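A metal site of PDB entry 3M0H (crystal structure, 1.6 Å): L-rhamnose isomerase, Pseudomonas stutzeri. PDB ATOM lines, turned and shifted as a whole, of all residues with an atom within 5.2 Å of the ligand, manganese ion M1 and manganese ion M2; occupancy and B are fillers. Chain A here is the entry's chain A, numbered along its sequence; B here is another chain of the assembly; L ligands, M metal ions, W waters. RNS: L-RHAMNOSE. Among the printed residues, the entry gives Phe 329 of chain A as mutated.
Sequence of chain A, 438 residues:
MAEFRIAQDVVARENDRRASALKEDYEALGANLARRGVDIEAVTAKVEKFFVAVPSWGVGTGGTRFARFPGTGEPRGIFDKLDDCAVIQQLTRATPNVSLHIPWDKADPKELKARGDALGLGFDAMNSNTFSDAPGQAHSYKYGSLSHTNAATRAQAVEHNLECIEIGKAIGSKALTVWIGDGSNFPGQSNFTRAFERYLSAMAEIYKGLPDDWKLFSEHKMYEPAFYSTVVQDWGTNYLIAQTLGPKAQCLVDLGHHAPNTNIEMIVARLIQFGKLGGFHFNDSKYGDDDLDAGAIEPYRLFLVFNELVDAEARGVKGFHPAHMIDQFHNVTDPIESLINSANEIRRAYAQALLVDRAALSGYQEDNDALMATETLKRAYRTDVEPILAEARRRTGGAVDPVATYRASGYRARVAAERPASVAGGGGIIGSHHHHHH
Water W2 bridges O4 of the ligand (2.7 Å) and OD2 of Asp 291 (2.7 Å). Water W3 lies within hydrogen-bond range of OD1 of Asp 291 (2.5 Å) and OD1 of Asp 254 (3.4 Å). Water W1 bridges an oxygen (O5) of the ligand (2.7 Å) and the side-chain amide oxygen of Asn 127 (2.8 Å).
Of the 20 residues printed, 5 come within 4 Å of manganese ion M1. The nearest printed residue that does not touch manganese ion M1 is Leu 252 (5.0 Å).
Residues that only touch manganese ion M2: Lys 221 (3.8 Å). Along chain A the residues within 4 Å of manganese ion M2 span positions 221 to 289.
The backbone carbonyl oxygen (O) of Asp 289 lies within hydrogen-bond range of the guanidinium group (NH2) of Arg 65 of chain B (3.1 Å). NE1 of Trp 57 lies within hydrogen-bond range of OD1 of Asp 327, at 2.9 Å. The side-chain amino group (NZ) of Lys 221 lies close to the side-chain carboxylate (OD2) of Asp 289, at 3.2 Å. The side-chain amino group (NZ) of Lys 221 lies within salt-bridge range of the side-chain carboxylate (OE1) of Glu 224, at 3.1 Å.
A ring nitrogen (NE2) of His 101 is in hydrogen-bond range of an oxygen (O5) of the ligand, at 2.8 Å. NZ of Lys 221 lies close to O1 of the ligand (2.7 Å).
Manganese ion M1 is bound by OD2 of Asp 327 (2.0 Å), OE2 of Glu 219 (2.1 Å), OD2 of Asp 254 (2.2 Å), O2 of the ligand (2.2 Å), ND1 of His 281 (2.2 Å) and O3 of the ligand (2.3 Å). Manganese ion M1 has six donor atoms within binding distance.
Manganese ion M2 is bound by water W3 (1.9 Å), O2 of the ligand (2.1 Å), water W2 (2.1 Å), NE2 of His 257 (2.1 Å), OD2 of Asp 289 (2.2 Å) and O1 of the ligand (2.2 Å). Manganese ion M2 has six donor atoms within binding distance.
Residues that only touch the ligand: Trp 179, Phe 66 of chain B and Trp 57. Hydrophobic or aromatic side chains that line the ligand: Trp 57, His 101, Trp 179, His 257, His 281 and Phe 66 of chain B.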
ATOM      1  N   TRP A  57       7.042   2.978 -10.834  1.00  0.00           N
ATOM      2  CA  TRP A  57       8.313   2.285 -10.881  1.00  0.00           C
ATOM      3  C   TRP A  57       9.515   3.202 -10.629  1.00  0.00           C
ATOM      4  O   TRP A  57      10.659   2.741 -10.556  1.00  0.00           O
ATOM      5  CB  TRP A  57       8.470   1.572 -12.232  1.00  0.00           C
ATOM      6  CG  TRP A  57       8.436   2.477 -13.430  1.00  0.00           C
ATOM      7  CD1 TRP A  57       9.497   3.081 -14.027  1.00  0.00           C
ATOM      8  CD2 TRP A  57       7.276   2.881 -14.162  1.00  0.00           C
ATOM      9  NE1 TRP A  57       9.080   3.818 -15.105  1.00  0.00           N
ATOM     10  CE2 TRP A  57       7.714   3.716 -15.216  1.00  0.00           C
ATOM     11  CE3 TRP A  57       5.910   2.596 -14.051  1.00  0.00           C
ATOM     12  CZ2 TRP A  57       6.840   4.292 -16.143  1.00  0.00           C
ATOM     13  CZ3 TRP A  57       5.032   3.175 -14.969  1.00  0.00           C
ATOM     14  CH2 TRP A  57       5.507   4.004 -16.002  1.00  0.00           C
ATOM     15  N   HIS A 101       1.913   0.185 -13.455  1.00  0.00           N
ATOM     16  CA  HIS A 101       2.524  -0.816 -14.317  1.00  0.00           C
ATOM     17  C   HIS A 101       2.051  -2.190 -13.843  1.00  0.00           C
ATOM     18  O   HIS A 101       2.196  -2.530 -12.673  1.00  0.00           O
ATOM     19  CB  HIS A 101       4.053  -0.713 -14.218  1.00  0.00           C
ATOM     20  CG  HIS A 101       4.758  -0.986 -15.509  1.00  0.00           C
ATOM     21  ND1 HIS A 101       4.684  -2.195 -16.162  1.00  0.00           N
ATOM     22  CD2 HIS A 101       5.545  -0.180 -16.272  1.00  0.00           C
ATOM     23  CE1 HIS A 101       5.391  -2.136 -17.283  1.00  0.00           C
ATOM     24  NE2 HIS A 101       5.923  -0.924 -17.371  1.00  0.00           N
ATOM     25  N   TRP A 104       3.470  -5.433 -11.915  1.00  0.00           N
ATOM     26  CA  TRP A 104       4.176  -4.920 -10.743  1.00  0.00           C
ATOM     27  C   TRP A 104       3.241  -4.318  -9.703  1.00  0.00           C
ATOM     28  O   TRP A 104       3.369  -4.588  -8.510  1.00  0.00           O
ATOM     29  CB  TRP A 104       5.208  -3.848 -11.118  1.00  0.00           C
ATOM     30  CG  TRP A 104       6.343  -4.318 -11.979  1.00  0.00           C
ATOM     31  CD1 TRP A 104       6.795  -5.602 -12.116  1.00  0.00           C
ATOM     32  CD2 TRP A 104       7.176  -3.502 -12.805  1.00  0.00           C
ATOM     33  NE1 TRP A 104       7.863  -5.635 -12.975  1.00  0.00           N
ATOM     34  CE2 TRP A 104       8.121  -4.355 -13.414  1.00  0.00           C
ATOM     35  CE3 TRP A 104       7.234  -2.133 -13.083  1.00  0.00           C
ATOM     36  CZ2 TRP A 104       9.106  -3.884 -14.294  1.00  0.00           C
ATOM     37  CZ3 TRP A 104       8.203  -1.656 -13.961  1.00  0.00           C
ATOM     38  CH2 TRP A 104       9.128  -2.538 -14.557  1.00  0.00           C
ATOM     39  N   ASN A 127       0.240   0.799 -17.934  1.00  0.00           N
ATOM     40  CA  ASN A 127       1.411   0.301 -18.648  1.00  0.00           C
ATOM     41  C   ASN A 127       1.426  -1.217 -18.560  1.00  0.00           C
ATOM     42  O   ASN A 127       1.387  -1.785 -17.467  1.00  0.00           O
ATOM     43  CB  ASN A 127       2.690   0.871 -18.025  1.00  0.00           C
ATOM     44  CG  ASN A 127       2.828   2.366 -18.217  1.00  0.00           C
ATOM     45  OD1 ASN A 127       3.390   2.823 -19.208  1.00  0.00           O
ATOM     46  ND2 ASN A 127       2.296   3.134 -17.275  1.00  0.00           N
ATOM     47  N   SER A 128       1.477  -1.883 -19.710  1.00  0.00           N
ATOM     48  CA  SER A 128       1.513  -3.337 -19.742  1.00  0.00           C
ATOM     49  C   SER A 128       2.952  -3.831 -19.663  1.00  0.00           C
ATOM     50  O   SER A 128       3.884  -3.071 -19.911  1.00  0.00           O
ATOM     51  CB  SER A 128       0.849  -3.857 -21.021  1.00  0.00           C
ATOM     52  OG  SER A 128       1.411  -3.255 -22.173  1.00  0.00           O
ATOM     53  N   PHE A 131       7.622  -7.755 -21.367  1.00  0.00           N
ATOM     54  CA  PHE A 131       9.053  -7.713 -21.625  1.00  0.00           C
ATOM     55  C   PHE A 131       9.777  -8.502 -20.539  1.00  0.00           C
ATOM     56  O   PHE A 131      11.013  -8.477 -20.439  1.00  0.00           O
ATOM     57  CB  PHE A 131       9.553  -6.251 -21.682  1.00  0.00           C
ATOM     58  CG  PHE A 131       9.177  -5.417 -20.487  1.00  0.00           C
ATOM     59  CD1 PHE A 131       9.878  -5.531 -19.291  1.00  0.00           C
ATOM     60  CD2 PHE A 131       8.140  -4.484 -20.567  1.00  0.00           C
ATOM     61  CE1 PHE A 131       9.560  -4.731 -18.195  1.00  0.00           C
ATOM     62  CE2 PHE A 131       7.819  -3.675 -19.477  1.00  0.00           C
ATOM     63  CZ  PHE A 131       8.524  -3.793 -18.289  1.00  0.00           C
ATOM     64  N   TRP A 179       4.822  -0.701 -24.379  1.00  0.00           N
ATOM     65  CA  TRP A 179       6.227  -0.711 -24.736  1.00  0.00           C
ATOM     66  C   TRP A 179       6.664  -2.158 -24.547  1.00  0.00           C
ATOM     67  O   TRP A 179       6.438  -2.746 -23.492  1.00  0.00           O
ATOM     68  CB  TRP A 179       7.094   0.161 -23.832  1.00  0.00           C
ATOM     69  CG  TRP A 179       8.567  -0.070 -24.142  1.00  0.00           C
ATOM     70  CD1 TRP A 179       9.245   0.349 -25.249  1.00  0.00           C
ATOM     71  CD2 TRP A 179       9.480  -0.905 -23.405  1.00  0.00           C
ATOM     72  NE1 TRP A 179      10.518  -0.178 -25.264  1.00  0.00           N
ATOM     73  CE2 TRP A 179      10.677  -0.950 -24.147  1.00  0.00           C
ATOM     74  CE3 TRP A 179       9.389  -1.630 -22.208  1.00  0.00           C
ATOM     75  CZ2 TRP A 179      11.797  -1.692 -23.721  1.00  0.00           C
ATOM     76  CZ3 TRP A 179      10.496  -2.353 -21.782  1.00  0.00           C
ATOM     77  CH2 TRP A 179      11.685  -2.382 -22.534  1.00  0.00           C
ATOM     78  N   GLU A 219       5.007   2.939 -27.757  1.00  0.00           N
ATOM     79  CA  GLU A 219       6.281   3.615 -27.472  1.00  0.00           C
ATOM     80  C   GLU A 219       7.462   3.007 -28.222  1.00  0.00           C
ATOM     81  O   GLU A 219       7.821   1.856 -27.995  1.00  0.00           O
ATOM     82  CB  GLU A 219       6.524   3.572 -25.965  1.00  0.00           C
ATOM     83  CG  GLU A 219       7.813   4.218 -25.496  1.00  0.00           C
ATOM     84  CD  GLU A 219       8.004   4.129 -23.998  1.00  0.00           C
ATOM     85  OE1 GLU A 219       7.225   3.413 -23.324  1.00  0.00           O
ATOM     86  OE2 GLU A 219       8.936   4.771 -23.481  1.00  0.00           O
ATOM     87  N   LYS A 221      11.484   2.579 -29.463  1.00  0.00           N
ATOM     88  CA  LYS A 221      12.791   2.560 -28.803  1.00  0.00           C
ATOM     89  C   LYS A 221      13.803   1.946 -29.765  1.00  0.00           C
ATOM     90  O   LYS A 221      13.591   0.854 -30.283  1.00  0.00           O
ATOM     91  CB  LYS A 221      12.725   1.751 -27.515  1.00  0.00           C
ATOM     92  CG  LYS A 221      13.953   1.930 -26.627  1.00  0.00           C
ATOM     93  CD  LYS A 221      13.854   1.136 -25.348  1.00  0.00           C
ATOM     94  CE  LYS A 221      15.043   1.419 -24.449  1.00  0.00           C
ATOM     95  NZ  LYS A 221      15.023   0.578 -23.207  1.00  0.00           N
ATOM     96  N   GLU A 224      17.645  -1.977 -26.866  1.00  0.00           N
ATOM     97  CA  GLU A 224      17.592  -2.400 -25.457  1.00  0.00           C
ATOM     98  C   GLU A 224      16.146  -2.685 -25.056  1.00  0.00           C
ATOM     99  O   GLU A 224      15.321  -1.782 -24.996  1.00  0.00           O
ATOM    100  CB  GLU A 224      18.188  -1.351 -24.496  1.00  0.00           C
ATOM    101  CG  GLU A 224      18.214  -1.880 -23.055  1.00  0.00           C
ATOM    102  CD  GLU A 224      18.399  -0.808 -22.000  1.00  0.00           C
ATOM    103  OE1 GLU A 224      17.921   0.325 -22.196  1.00  0.00           O
ATOM    104  OE2 GLU A 224      19.011  -1.119 -20.951  1.00  0.00           O
ATOM    105  N   LEU A 252       3.865   7.521 -28.437  1.00  0.00           N
ATOM    106  CA  LEU A 252       4.439   8.084 -27.219  1.00  0.00           C
ATOM    107  C   LEU A 252       5.934   8.258 -27.448  1.00  0.00           C
ATOM    108  O   LEU A 252       6.609   7.336 -27.918  1.00  0.00           O
ATOM    109  CB  LEU A 252       4.175   7.162 -26.021  1.00  0.00           C
ATOM    110  CG  LEU A 252       4.629   7.729 -24.676  1.00  0.00           C
ATOM    111  CD1 LEU A 252       3.603   7.430 -23.599  1.00  0.00           C
ATOM    112  CD2 LEU A 252       5.992   7.162 -24.324  1.00  0.00           C
ATOM    113  N   ASP A 254       9.539   8.928 -25.843  1.00  0.00           N
ATOM    114  CA  ASP A 254      10.371   8.858 -24.646  1.00  0.00           C
ATOM    115  C   ASP A 254      11.683   9.496 -25.096  1.00  0.00           C
ATOM    116  O   ASP A 254      12.354   8.993 -25.986  1.00  0.00           O
ATOM    117  CB  ASP A 254      10.585   7.403 -24.223  1.00  0.00           C
ATOM    118  CG  ASP A 254      11.371   7.277 -22.934  1.00  0.00           C
ATOM    119  OD1 ASP A 254      12.452   7.888 -22.850  1.00  0.00           O
ATOM    120  OD2 ASP A 254      10.920   6.575 -22.007  1.00  0.00           O
ATOM    121  N   HIS A 257      15.000   7.485 -26.053  1.00  0.00           N
ATOM    122  CA  HIS A 257      14.887   6.349 -26.964  1.00  0.00           C
ATOM    123  C   HIS A 257      15.297   6.589 -28.408  1.00  0.00           C
ATOM    124  O   HIS A 257      14.889   5.859 -29.315  1.00  0.00           O
ATOM    125  CB  HIS A 257      13.448   5.829 -26.954  1.00  0.00           C
ATOM    126  CG  HIS A 257      13.049   5.179 -25.667  1.00  0.00           C
ATOM    127  ND1 HIS A 257      11.885   4.453 -25.536  1.00  0.00           N
ATOM    128  CD2 HIS A 257      13.660   5.122 -24.467  1.00  0.00           C
ATOM    129  CE1 HIS A 257      11.803   3.974 -24.309  1.00  0.00           C
ATOM    130  NE2 HIS A 257      12.867   4.372 -23.634  1.00  0.00           N
ATOM    131  N   HIS A 281       7.351  10.699 -22.403  1.00  0.00           N
ATOM    132  CA  HIS A 281       7.971  10.010 -21.277  1.00  0.00           C
ATOM    133  C   HIS A 281       9.215  10.874 -21.102  1.00  0.00           C
ATOM    134  O   HIS A 281      10.153  10.795 -21.902  1.00  0.00           O
ATOM    135  CB  HIS A 281       8.349   8.579 -21.619  1.00  0.00           C
ATOM    136  CG  HIS A 281       7.320   7.561 -21.204  1.00  0.00           C
ATOM    137  ND1 HIS A 281       7.579   6.213 -21.177  1.00  0.00           N
ATOM    138  CD2 HIS A 281       6.039   7.714 -20.791  1.00  0.00           C
ATOM    139  CE1 HIS A 281       6.496   5.564 -20.774  1.00  0.00           C
ATOM    140  NE2 HIS A 281       5.551   6.453 -20.533  1.00  0.00           N
ATOM    141  N   ASP A 289      19.583   5.044 -23.240  1.00  0.00           N
ATOM    142  CA  ASP A 289      18.330   5.287 -22.530  1.00  0.00           C
ATOM    143  C   ASP A 289      18.691   5.300 -21.056  1.00  0.00           C
ATOM    144  O   ASP A 289      18.297   4.424 -20.283  1.00  0.00           O
ATOM    145  CB  ASP A 289      17.323   4.179 -22.836  1.00  0.00           C
ATOM    146  CG  ASP A 289      15.993   4.413 -22.196  1.00  0.00           C
ATOM    147  OD1 ASP A 289      15.624   5.600 -22.016  1.00  0.00           O
ATOM    148  OD2 ASP A 289      15.304   3.418 -21.867  1.00  0.00           O
ATOM    149  N   ASP A 291      17.731   7.157 -18.605  1.00  0.00           N
ATOM    150  CA  ASP A 291      16.630   7.386 -17.659  1.00  0.00           C
ATOM    151  C   ASP A 291      16.988   8.271 -16.471  1.00  0.00           C
ATOM    152  O   ASP A 291      16.540   8.030 -15.340  1.00  0.00           O
ATOM    153  CB  ASP A 291      16.074   6.050 -17.158  1.00  0.00           C
ATOM    154  CG  ASP A 291      15.193   5.365 -18.188  1.00  0.00           C
ATOM    155  OD1 ASP A 291      14.379   6.075 -18.816  1.00  0.00           O
ATOM    156  OD2 ASP A 291      15.309   4.127 -18.357  1.00  0.00           O
ATOM    157  N   ASP A 327       9.363   9.148 -16.927  1.00  0.00           N
ATOM    158  CA  ASP A 327       9.774   7.750 -16.982  1.00  0.00           C
ATOM    159  C   ASP A 327      11.252   7.787 -16.683  1.00  0.00           C
ATOM    160  O   ASP A 327      12.072   8.000 -17.582  1.00  0.00           O
ATOM    161  CB  ASP A 327       9.537   7.127 -18.351  1.00  0.00           C
ATOM    162  CG  ASP A 327       9.990   5.671 -18.411  1.00  0.00           C
ATOM    163  OD1 ASP A 327      10.364   5.126 -17.344  1.00  0.00           O
ATOM    164  OD2 ASP A 327       9.978   5.076 -19.501  1.00  0.00           O
ATOM    165  N   PHE A 329      14.515   6.248 -13.762  1.00  0.00           N
ATOM    166  CA  PHE A 329      14.961   5.285 -12.773  1.00  0.00           C
ATOM    167  C   PHE A 329      16.019   6.028 -11.984  1.00  0.00           C
ATOM    168  O   PHE A 329      16.871   6.713 -12.563  1.00  0.00           O
ATOM    169  CB  PHE A 329      15.528   4.032 -13.443  1.00  0.00           C
ATOM    170  CG  PHE A 329      14.473   3.101 -13.959  1.00  0.00           C
ATOM    171  CD1 PHE A 329      13.725   2.325 -13.081  1.00  0.00           C
ATOM    172  CD2 PHE A 329      14.188   3.046 -15.319  1.00  0.00           C
ATOM    173  CE1 PHE A 329      12.713   1.497 -13.556  1.00  0.00           C
ATOM    174  CE2 PHE A 329      13.176   2.219 -15.794  1.00  0.00           C
ATOM    175  CZ  PHE A 329      12.436   1.448 -14.914  1.00  0.00           C
ATOM    176  N   ARG B  65      18.734  -5.188 -17.917  1.00  0.00           N
ATOM    177  CA  ARG B  65      18.128  -4.658 -16.697  1.00  0.00           C
ATOM    178  C   ARG B  65      16.624  -4.908 -16.679  1.00  0.00           C
ATOM    179  O   ARG B  65      15.989  -4.796 -15.635  1.00  0.00           O
ATOM    180  CB  ARG B  65      18.396  -3.163 -16.552  1.00  0.00           C
ATOM    181  CG  ARG B  65      17.901  -2.322 -17.708  1.00  0.00           C
ATOM    182  CD  ARG B  65      18.013  -0.830 -17.416  1.00  0.00           C
ATOM    183  NE  ARG B  65      17.731  -0.049 -18.620  1.00  0.00           N
ATOM    184  CZ  ARG B  65      17.092   1.118 -18.650  1.00  0.00           C
ATOM    185  NH1 ARG B  65      16.650   1.675 -17.524  1.00  0.00           N
ATOM    186  NH2 ARG B  65      16.878   1.715 -19.810  1.00  0.00           N
ATOM    187  N   PHE B  66      16.063  -5.263 -17.828  1.00  0.00           N
ATOM    188  CA  PHE B  66      14.626  -5.515 -17.930  1.00  0.00           C
ATOM    189  C   PHE B  66      14.213  -6.959 -17.613  1.00  0.00           C
ATOM    190  O   PHE B  66      13.123  -7.176 -17.082  1.00  0.00           O
ATOM    191  CB  PHE B  66      14.120  -5.149 -19.325  1.00  0.00           C
ATOM    192  CG  PHE B  66      14.137  -3.684 -19.601  1.00  0.00           C
ATOM    193  CD1 PHE B  66      13.192  -2.843 -19.011  1.00  0.00           C
ATOM    194  CD2 PHE B  66      15.127  -3.122 -20.406  1.00  0.00           C
ATOM    195  CE1 PHE B  66      13.229  -1.466 -19.220  1.00  0.00           C
ATOM    196  CE2 PHE B  66      15.177  -1.743 -20.621  1.00  0.00           C
ATOM    197  CZ  PHE B  66      14.220  -0.921 -20.030  1.00  0.00           C
HETATM  198  C1  RNS L   1      11.531   1.093 -21.688  1.00  0.00           C
HETATM  199  C2  RNS L   1      10.465   2.175 -21.816  1.00  0.00           C
HETATM  200  C3  RNS L   1       9.278   1.878 -20.903  1.00  0.00           C
HETATM  201  C4  RNS L   1       9.698   1.483 -19.481  1.00  0.00           C
HETATM  202  C5  RNS L   1       8.468   1.415 -18.582  1.00  0.00           C
HETATM  203  C6  RNS L   1       8.886   0.930 -17.198  1.00  0.00           C
HETATM  204  O1  RNS L   1      12.688   1.332 -22.039  1.00  0.00           O
HETATM  205  O2  RNS L   1      11.028   3.434 -21.493  1.00  0.00           O
HETATM  206  O3  RNS L   1       8.429   3.017 -20.862  1.00  0.00           O
HETATM  207  O4  RNS L   1      10.631   2.429 -18.961  1.00  0.00           O
HETATM  208  O5  RNS L   1       7.527   0.511 -19.134  1.00  0.00           O
HETATM  209 MN    MN M   1       9.468   5.024 -21.435  1.00  0.00          MN
HETATM  210 MN    MN M   2      13.113   3.487 -21.712  1.00  0.00          MN
HETATM  211  O   HOH W   1       5.438   1.397 -20.548  1.00  0.00           O
HETATM  212  O   HOH W   2      13.214   2.931 -19.669  1.00  0.00           O
HETATM  213  O   HOH W   3      13.539   5.233 -21.029  1.00  0.00           O
